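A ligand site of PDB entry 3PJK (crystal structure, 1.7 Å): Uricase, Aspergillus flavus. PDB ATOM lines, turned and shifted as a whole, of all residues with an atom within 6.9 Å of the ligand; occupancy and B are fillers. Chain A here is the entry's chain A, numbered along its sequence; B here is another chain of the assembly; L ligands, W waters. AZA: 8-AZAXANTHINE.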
ATOM      1  N   SER A 158      11.775  21.030 -23.488  1.00  0.00           N
ATOM      2  CA  SER A 158      10.349  21.155 -23.333  1.00  0.00           C
ATOM      3  C   SER A 158       9.897  21.951 -24.548  1.00  0.00           C
ATOM      4  O   SER A 158      10.556  22.916 -24.952  1.00  0.00           O
ATOM      5  CB  SER A 158      10.006  21.913 -22.050  1.00  0.00           C
ATOM      6  OG  SER A 158       8.614  22.235 -22.023  1.00  0.00           O
ATOM      7  N   GLN A 159       8.797  21.492 -25.155  1.00  0.00           N
ATOM      8  CA  GLN A 159       8.217  22.115 -26.325  1.00  0.00           C
ATOM      9  C   GLN A 159       6.742  22.302 -26.097  1.00  0.00           C
ATOM     10  O   GLN A 159       6.135  21.626 -25.255  1.00  0.00           O
ATOM     11  CB  GLN A 159       8.382  21.207 -27.568  1.00  0.00           C
ATOM     12  CG  GLN A 159       9.808  20.662 -27.704  1.00  0.00           C
ATOM     13  CD  GLN A 159      10.046  19.898 -29.007  1.00  0.00           C
ATOM     14  OE1 GLN A 159       9.111  19.570 -29.747  1.00  0.00           O
ATOM     15  NE2 GLN A 159      11.315  19.645 -29.285  1.00  0.00           N
ATOM     16  N   PHE A 160       6.142  23.167 -26.893  1.00  0.00           N
ATOM     17  CA  PHE A 160       4.709  23.272 -26.915  1.00  0.00           C
ATOM     18  C   PHE A 160       4.239  23.892 -28.228  1.00  0.00           C
ATOM     19  O   PHE A 160       4.279  25.107 -28.405  1.00  0.00           O
ATOM     20  CB  PHE A 160       4.135  24.026 -25.672  1.00  0.00           C
ATOM     21  CG  PHE A 160       2.651  23.893 -25.539  1.00  0.00           C
ATOM     22  CD1 PHE A 160       2.070  22.637 -25.320  1.00  0.00           C
ATOM     23  CD2 PHE A 160       1.817  25.014 -25.674  1.00  0.00           C
ATOM     24  CE1 PHE A 160       0.668  22.502 -25.235  1.00  0.00           C
ATOM     25  CE2 PHE A 160       0.415  24.892 -25.584  1.00  0.00           C
ATOM     26  CZ  PHE A 160      -0.151  23.613 -25.383  1.00  0.00           C
ATOM     27  N   PHE A 163      -1.034  23.332 -30.854  1.00  0.00           N
ATOM     28  CA  PHE A 163      -2.293  23.551 -30.140  1.00  0.00           C
ATOM     29  C   PHE A 163      -3.334  24.301 -30.989  1.00  0.00           C
ATOM     30  O   PHE A 163      -3.007  24.871 -32.038  1.00  0.00           O
ATOM     31  CB  PHE A 163      -2.066  24.273 -28.787  1.00  0.00           C
ATOM     32  CG  PHE A 163      -1.194  25.491 -28.904  1.00  0.00           C
ATOM     33  CD1 PHE A 163       0.183  25.374 -28.794  1.00  0.00           C
ATOM     34  CD2 PHE A 163      -1.754  26.761 -29.125  1.00  0.00           C
ATOM     35  CE1 PHE A 163       1.030  26.472 -28.912  1.00  0.00           C
ATOM     36  CE2 PHE A 163      -0.909  27.885 -29.234  1.00  0.00           C
ATOM     37  CZ  PHE A 163       0.470  27.729 -29.138  1.00  0.00           C
ATOM     38  N   LEU A 171      -0.642  33.054 -28.139  1.00  0.00           N
ATOM     39  CA  LEU A 171       0.549  32.295 -27.752  1.00  0.00           C
ATOM     40  C   LEU A 171       1.301  31.772 -28.984  1.00  0.00           C
ATOM     41  O   LEU A 171       0.686  31.150 -29.849  1.00  0.00           O
ATOM     42  CB  LEU A 171       0.140  31.110 -26.866  1.00  0.00           C
ATOM     43  CG  LEU A 171       1.295  30.217 -26.359  1.00  0.00           C
ATOM     44  CD1 LEU A 171       2.181  30.988 -25.368  1.00  0.00           C
ATOM     45  CD2 LEU A 171       0.729  28.950 -25.707  1.00  0.00           C
ATOM     46  N   ARG A 177      11.540  25.657 -24.521  1.00  0.00           N
ATOM     47  CA  ARG A 177      11.103  26.548 -23.432  1.00  0.00           C
ATOM     48  C   ARG A 177      11.549  25.988 -22.100  1.00  0.00           C
ATOM     49  O   ARG A 177      11.974  24.829 -21.997  1.00  0.00           O
ATOM     50  CB  ARG A 177       9.582  26.731 -23.432  1.00  0.00           C
ATOM     51  CG  ARG A 177       8.842  25.432 -23.091  1.00  0.00           C
ATOM     52  CD  ARG A 177       7.342  25.592 -23.087  1.00  0.00           C
ATOM     53  NE  ARG A 177       6.697  24.347 -22.613  1.00  0.00           N
ATOM     54  CZ  ARG A 177       5.411  24.231 -22.289  1.00  0.00           C
ATOM     55  NH1 ARG A 177       4.567  25.255 -22.449  1.00  0.00           N
ATOM     56  NH2 ARG A 177       4.946  23.046 -21.855  1.00  0.00           N
ATOM     57  N   LEU A 179      10.591  24.630 -18.428  1.00  0.00           N
ATOM     58  CA  LEU A 179       9.445  23.995 -17.770  1.00  0.00           C
ATOM     59  C   LEU A 179       9.713  23.881 -16.279  1.00  0.00           C
ATOM     60  O   LEU A 179      10.698  23.295 -15.855  1.00  0.00           O
ATOM     61  CB  LEU A 179       9.187  22.602 -18.387  1.00  0.00           C
ATOM     62  CG  LEU A 179       8.039  21.764 -17.834  1.00  0.00           C
ATOM     63  CD1 LEU A 179       6.720  22.532 -17.950  1.00  0.00           C
ATOM     64  CD2 LEU A 179       7.977  20.422 -18.610  1.00  0.00           C
ATOM     65  N   SER A 225       9.706  16.892 -23.584  1.00  0.00           N
ATOM     66  CA  SER A 225       8.302  17.027 -23.264  1.00  0.00           C
ATOM     67  C   SER A 225       7.515  17.729 -24.345  1.00  0.00           C
ATOM     68  O   SER A 225       7.862  18.828 -24.787  1.00  0.00           O
ATOM     69  CB  SER A 225       8.182  17.772 -21.917  1.00  0.00           C
ATOM     70  OG  SER A 225       6.823  18.105 -21.681  1.00  0.00           O
ATOM     71  N   ALA A 226       6.440  17.093 -24.769  1.00  0.00           N
ATOM     72  CA  ALA A 226       5.550  17.653 -25.760  1.00  0.00           C
ATOM     73  C   ALA A 226       4.498  18.583 -25.159  1.00  0.00           C
ATOM     74  O   ALA A 226       3.886  19.381 -25.874  1.00  0.00           O
ATOM     75  CB  ALA A 226       4.844  16.498 -26.515  1.00  0.00           C
ATOM     76  N   SER A 227       4.297  18.477 -23.837  1.00  0.00           N
ATOM     77  CA  SER A 227       3.336  19.285 -23.093  1.00  0.00           C
ATOM     78  C   SER A 227       3.432  18.778 -21.660  1.00  0.00           C
ATOM     79  O   SER A 227       3.994  17.704 -21.421  1.00  0.00           O
ATOM     80  CB  SER A 227       1.887  19.102 -23.572  1.00  0.00           C
ATOM     81  OG  SER A 227       1.454  17.739 -23.412  1.00  0.00           O
ATOM     82  N   VAL A 228       2.854  19.536 -20.725  1.00  0.00           N
ATOM     83  CA  VAL A 228       2.805  19.036 -19.353  1.00  0.00           C
ATOM     84  C   VAL A 228       1.941  17.779 -19.336  1.00  0.00           C
ATOM     85  O   VAL A 228       2.255  16.792 -18.657  1.00  0.00           O
ATOM     86  CB  VAL A 228       2.235  20.125 -18.415  1.00  0.00           C
ATOM     87  CG1 VAL A 228       1.994  19.571 -17.023  1.00  0.00           C
ATOM     88  CG2 VAL A 228       3.217  21.317 -18.383  1.00  0.00           C
ATOM     89  N   GLN A 229       0.843  17.837 -20.086  1.00  0.00           N
ATOM     90  CA  GLN A 229      -0.112  16.715 -20.207  1.00  0.00           C
ATOM     91  C   GLN A 229       0.594  15.400 -20.557  1.00  0.00           C
ATOM     92  O   GLN A 229       0.411  14.357 -19.870  1.00  0.00           O
ATOM     93  CB  GLN A 229      -1.200  17.035 -21.246  1.00  0.00           C
ATOM     94  CG  GLN A 229      -2.248  18.092 -20.812  1.00  0.00           C
ATOM     95  CD  GLN A 229      -1.827  19.522 -21.097  1.00  0.00           C
ATOM     96  OE1 GLN A 229      -0.635  19.849 -21.181  1.00  0.00           O
ATOM     97  NE2 GLN A 229      -2.826  20.383 -21.242  1.00  0.00           N
ATOM     98  N   ALA A 230       1.421  15.434 -21.615  1.00  0.00           N
ATOM     99  CA  ALA A 230       2.038  14.215 -22.117  1.00  0.00           C
ATOM    100  C   ALA A 230       3.078  13.674 -21.140  1.00  0.00           C
ATOM    101  O   ALA A 230       3.192  12.456 -20.932  1.00  0.00           O
ATOM    102  CB  ALA A 230       2.653  14.452 -23.500  1.00  0.00           C
ATOM    103  N   ASN A 255       1.956  25.043 -14.189  1.00  0.00           N
ATOM    104  CA  ASN A 255       2.970  25.340 -15.160  1.00  0.00           C
ATOM    105  C   ASN A 255       3.432  26.758 -14.796  1.00  0.00           C
ATOM    106  O   ASN A 255       2.708  27.692 -15.023  1.00  0.00           O
ATOM    107  CB  ASN A 255       2.366  25.251 -16.567  1.00  0.00           C
ATOM    108  CG  ASN A 255       3.415  25.396 -17.675  1.00  0.00           C
ATOM    109  OD1 ASN A 255       4.612  25.522 -17.406  1.00  0.00           O
ATOM    110  ND2 ASN A 255       2.953  25.409 -18.929  1.00  0.00           N
ATOM    111  N   HIS A 257       5.341  29.885 -15.300  1.00  0.00           N
ATOM    112  CA  HIS A 257       5.910  30.428 -16.534  1.00  0.00           C
ATOM    113  C   HIS A 257       7.167  31.282 -16.317  1.00  0.00           C
ATOM    114  O   HIS A 257       7.228  32.073 -15.388  1.00  0.00           O
ATOM    115  CB  HIS A 257       4.880  31.268 -17.274  1.00  0.00           C
ATOM    116  CG  HIS A 257       3.584  30.553 -17.486  1.00  0.00           C
ATOM    117  ND1 HIS A 257       3.503  29.397 -18.239  1.00  0.00           N
ATOM    118  CD2 HIS A 257       2.330  30.803 -17.028  1.00  0.00           C
ATOM    119  CE1 HIS A 257       2.243  28.976 -18.258  1.00  0.00           C
ATOM    120  NE2 HIS A 257       1.516  29.805 -17.521  1.00  0.00           N
ATOM    121  N   GLY A 287      -0.538  28.066 -15.429  1.00  0.00           N
ATOM    122  CA  GLY A 287      -1.322  26.929 -15.906  1.00  0.00           C
ATOM    123  C   GLY A 287      -1.528  25.963 -14.767  1.00  0.00           C
ATOM    124  O   GLY A 287      -0.736  25.918 -13.821  1.00  0.00           O
ATOM    125  N   ILE A 289      -2.680  21.829 -14.519  1.00  0.00           N
ATOM    126  CA  ILE A 289      -2.959  20.663 -15.375  1.00  0.00           C
ATOM    127  C   ILE A 289      -3.121  19.476 -14.473  1.00  0.00           C
ATOM    128  O   ILE A 289      -2.236  19.204 -13.655  1.00  0.00           O
ATOM    129  CB  ILE A 289      -1.756  20.378 -16.351  1.00  0.00           C
ATOM    130  CG1 ILE A 289      -1.219  21.674 -17.006  1.00  0.00           C
ATOM    131  CG2 ILE A 289      -2.207  19.333 -17.400  1.00  0.00           C
ATOM    132  CD1 ILE A 289      -2.201  22.438 -17.781  1.00  0.00           C
ATOM    133  N   TYR B   9      -7.858  20.854 -17.086  1.00  0.00           N
ATOM    134  CA  TYR B   9      -6.674  21.701 -17.196  1.00  0.00           C
ATOM    135  C   TYR B   9      -7.197  23.126 -17.487  1.00  0.00           C
ATOM    136  O   TYR B   9      -8.312  23.319 -17.966  1.00  0.00           O
ATOM    137  CB  TYR B   9      -5.719  21.188 -18.303  1.00  0.00           C
ATOM    138  CG  TYR B   9      -6.169  21.681 -19.639  1.00  0.00           C
ATOM    139  CD1 TYR B   9      -7.326  21.167 -20.227  1.00  0.00           C
ATOM    140  CD2 TYR B   9      -5.509  22.740 -20.264  1.00  0.00           C
ATOM    141  CE1 TYR B   9      -7.802  21.690 -21.436  1.00  0.00           C
ATOM    142  CE2 TYR B   9      -5.964  23.253 -21.465  1.00  0.00           C
ATOM    143  CZ  TYR B   9      -7.122  22.732 -22.034  1.00  0.00           C
ATOM    144  OH  TYR B   9      -7.579  23.268 -23.216  1.00  0.00           O
ATOM    145  N   GLY B  10      -6.342  24.112 -17.229  1.00  0.00           N
ATOM    146  CA  GLY B  10      -6.737  25.502 -17.428  1.00  0.00           C
ATOM    147  C   GLY B  10      -5.754  26.485 -16.810  1.00  0.00           C
ATOM    148  O   GLY B  10      -4.567  26.198 -16.690  1.00  0.00           O
ATOM    149  N   LYS B  11      -6.275  27.647 -16.429  1.00  0.00           N
ATOM    150  CA  LYS B  11      -5.421  28.732 -15.923  1.00  0.00           C
ATOM    151  C   LYS B  11      -5.905  29.104 -14.545  1.00  0.00           C
ATOM    152  O   LYS B  11      -7.110  29.266 -14.338  1.00  0.00           O
ATOM    153  CB  LYS B  11      -5.522  29.964 -16.839  1.00  0.00           C
ATOM    154  CG  LYS B  11      -4.298  30.891 -16.747  1.00  0.00           C
ATOM    155  CD  LYS B  11      -3.082  30.191 -17.338  1.00  0.00           C
ATOM    156  CE  LYS B  11      -2.052  31.094 -17.940  1.00  0.00           C
ATOM    157  NZ  LYS B  11      -1.013  30.297 -18.686  1.00  0.00           N
ATOM    158  N   ASN B  52      -1.626  17.746 -29.352  1.00  0.00           N
ATOM    159  CA  ASN B  52      -1.997  19.070 -28.837  1.00  0.00           C
ATOM    160  C   ASN B  52      -3.166  19.730 -29.557  1.00  0.00           C
ATOM    161  O   ASN B  52      -3.638  20.783 -29.136  1.00  0.00           O
ATOM    162  CB  ASN B  52      -0.780  20.007 -28.753  1.00  0.00           C
ATOM    163  CG  ASN B  52       0.225  19.546 -27.707  1.00  0.00           C
ATOM    164  OD1 ASN B  52      -0.133  18.835 -26.775  1.00  0.00           O
ATOM    165  ND2 ASN B  52       1.477  19.975 -27.857  1.00  0.00           N
ATOM    166  N   ILE B  55      -6.023  20.843 -27.517  1.00  0.00           N
ATOM    167  CA  ILE B  55      -5.802  21.779 -26.407  1.00  0.00           C
ATOM    168  C   ILE B  55      -6.098  23.222 -26.781  1.00  0.00           C
ATOM    169  O   ILE B  55      -5.462  23.752 -27.695  1.00  0.00           O
ATOM    170  CB  ILE B  55      -4.368  21.679 -25.850  1.00  0.00           C
ATOM    171  CG1 ILE B  55      -4.102  20.271 -25.284  1.00  0.00           C
ATOM    172  CG2 ILE B  55      -4.116  22.752 -24.720  1.00  0.00           C
ATOM    173  CD1 ILE B  55      -2.622  20.046 -24.918  1.00  0.00           C
ATOM    174  N   VAL B  56      -7.066  23.820 -26.081  1.00  0.00           N
ATOM    175  CA  VAL B  56      -7.254  25.270 -26.040  1.00  0.00           C
ATOM    176  C   VAL B  56      -6.147  25.711 -25.066  1.00  0.00           C
ATOM    177  O   VAL B  56      -6.189  25.319 -23.890  1.00  0.00           O
ATOM    178  CB  VAL B  56      -8.658  25.654 -25.512  1.00  0.00           C
ATOM    179  CG1 VAL B  56      -8.784  27.174 -25.367  1.00  0.00           C
ATOM    180  CG2 VAL B  56      -9.757  25.106 -26.460  1.00  0.00           C
ATOM    181  N   ALA B  57      -5.181  26.492 -25.546  1.00  0.00           N
ATOM    182  CA  ALA B  57      -3.996  26.802 -24.721  1.00  0.00           C
ATOM    183  C   ALA B  57      -4.442  27.545 -23.473  1.00  0.00           C
ATOM    184  O   ALA B  57      -5.390  28.327 -23.515  1.00  0.00           O
ATOM    185  CB  ALA B  57      -2.972  27.639 -25.496  1.00  0.00           C
ATOM    186  N   THR B  58      -3.773  27.280 -22.348  1.00  0.00           N
ATOM    187  CA  THR B  58      -4.204  27.950 -21.104  1.00  0.00           C
ATOM    188  C   THR B  58      -3.994  29.455 -21.249  1.00  0.00           C
ATOM    189  O   THR B  58      -4.743  30.225 -20.663  1.00  0.00           O
ATOM    190  CB  THR B  58      -3.434  27.457 -19.852  1.00  0.00           C
ATOM    191  OG1 THR B  58      -2.067  27.874 -19.934  1.00  0.00           O
ATOM    192  CG2 THR B  58      -3.533  25.904 -19.748  1.00  0.00           C
ATOM    193  N   ASP B  59      -2.990  29.855 -22.024  1.00  0.00           N
ATOM    194  CA  ASP B  59      -2.802  31.277 -22.339  1.00  0.00           C
ATOM    195  C   ASP B  59      -4.029  31.862 -23.026  1.00  0.00           C
ATOM    196  O   ASP B  59      -4.406  32.971 -22.749  1.00  0.00           O
ATOM    197  CB  ASP B  59      -1.573  31.485 -23.220  1.00  0.00           C
ATOM    198  CG  ASP B  59      -1.207  32.950 -23.358  1.00  0.00           C
ATOM    199  OD1 ASP B  59      -0.671  33.496 -22.377  1.00  0.00           O
ATOM    200  OD2 ASP B  59      -1.474  33.549 -24.440  1.00  0.00           O
ATOM    201  N   SER B  60      -4.652  31.090 -23.935  1.00  0.00           N
ATOM    202  CA  SER B  60      -5.924  31.528 -24.550  1.00  0.00           C
ATOM    203  C   SER B  60      -7.095  31.638 -23.582  1.00  0.00           C
ATOM    204  O   SER B  60      -7.953  32.515 -23.711  1.00  0.00           O
ATOM    205  CB  SER B  60      -6.289  30.602 -25.731  1.00  0.00           C
ATOM    206  OG  SER B  60      -5.150  30.511 -26.566  1.00  0.00           O
HETATM  207  N1  AZA L   1       0.108  22.667 -21.667  1.00  0.00           N
HETATM  208  C2  AZA L   1       1.393  23.102 -21.706  1.00  0.00           C
HETATM  209  O2  AZA L   1       2.280  22.249 -21.492  1.00  0.00           O
HETATM  210  N3  AZA L   1       1.744  24.404 -21.978  1.00  0.00           N
HETATM  211  C4  AZA L   1       0.748  25.269 -22.238  1.00  0.00           C
HETATM  212  C5  AZA L   1      -0.629  24.878 -22.233  1.00  0.00           C
HETATM  213  C6  AZA L   1      -0.930  23.471 -21.931  1.00  0.00           C
HETATM  214  O6  AZA L   1      -2.106  23.090 -21.865  1.00  0.00           O
HETATM  215  N7  AZA L   1      -1.421  25.954 -22.530  1.00  0.00           N
HETATM  216  N8  AZA L   1      -0.468  26.974 -22.712  1.00  0.00           N
HETATM  217  N9  AZA L   1       0.873  26.599 -22.538  1.00  0.00           N
HETATM  218  O   HOH W   1       2.997  28.260 -22.255  1.00  0.00           O
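The side-chain amide nitrogen of Gln 229 sits at hydrogen-bond distance from an oxygen (O6) of the ligand, at 2.9 Å. ND2 of Asn 255 lies close to N3 of the ligand, at 3.4 Å. The guanidinium group (NH2) of Arg 177 lies within hydrogen-bond range of an oxygen (O2) of the ligand (2.8 Å). The backbone NH (N) of Val 228 lies within hydrogen-bond range of an oxygen (O2) of the ligand, 2.9 Å away. N of Thr 58 of chain B is in hydrogen-bond range of N7 of the ligand, at 2.7 Å. The side-chain hydroxyl (OG1) of Thr 58 of chain B lies within hydrogen-bond range of a nitrogen (N7) of the ligand (3.3 Å).
The side-chain hydroxyl (OG) of Ser 227 sits at hydrogen-bond distance from the backbone NH (N) of Ala 230, 2.9 Å away. O of Asn 255 is in hydrogen-bond range of NE2 of His 257, at 3.5 Å. O of Val 56 of chain B is in hydrogen-bond range of OH of Tyr 9 of chain B. O of Gly 287 sits at hydrogen-bond distance from N of Asn 255 (2.9 Å). The backbone carbonyl oxygen of Ser 227 lies within hydrogen-bond range of the side-chain hydroxyl of Ser 225. NE of Arg 177 lies within hydrogen-bond range of OG of Ser 158, at 2.9 Å. N of Gln 229 lies close to OG of Ser 227 (3.4 Å). OG1 of Thr 58 of chain B lies within hydrogen-bond range of NZ of Lys 11 of chain B, 2.9 Å away.
Phe 160 touches the ligand (CE2 to C4, 3.4 Å). Leu 171 touches the ligand. Ser 227 touches the ligand. Tyr 9 of chain B touches the ligand (CD2 to O6, 3.8 Å). CG2 of Ile 55 of chain B touches O6 of the ligand (3.5 Å). CA of Ala 57 of chain B touches N7 of the ligand (3.5 Å). N of Asp 59 of chain B touches N8 of the ligand (3.9 Å). Hydrophobic or aromatic side chains within 4 Å of the ligand: Phe 160, Leu 171, Val 228, Tyr 9 of chain B, Ile 55 of chain B and Ala 57 of chain B. 12 residues have an atom within 4 Å of the ligand: Phe 160, Leu 171, Arg 177, Ser 227, Val 228, Gln 229, Asn 255, Tyr 9 of chain B, Ile 55 of chain B, Ala 57 of chain B, Thr 58 of chain B and Asp 59 of chain B. Along chain A the residues within 4 Å of the ligand span positions 160 to 255. The nearest printed residue that does not touch the ligand is Ile 289 (4.1 Å).
Water W1 bridges N9 of the ligand (2.7 Å) and NH1 of Arg 177 (3.4 Å).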
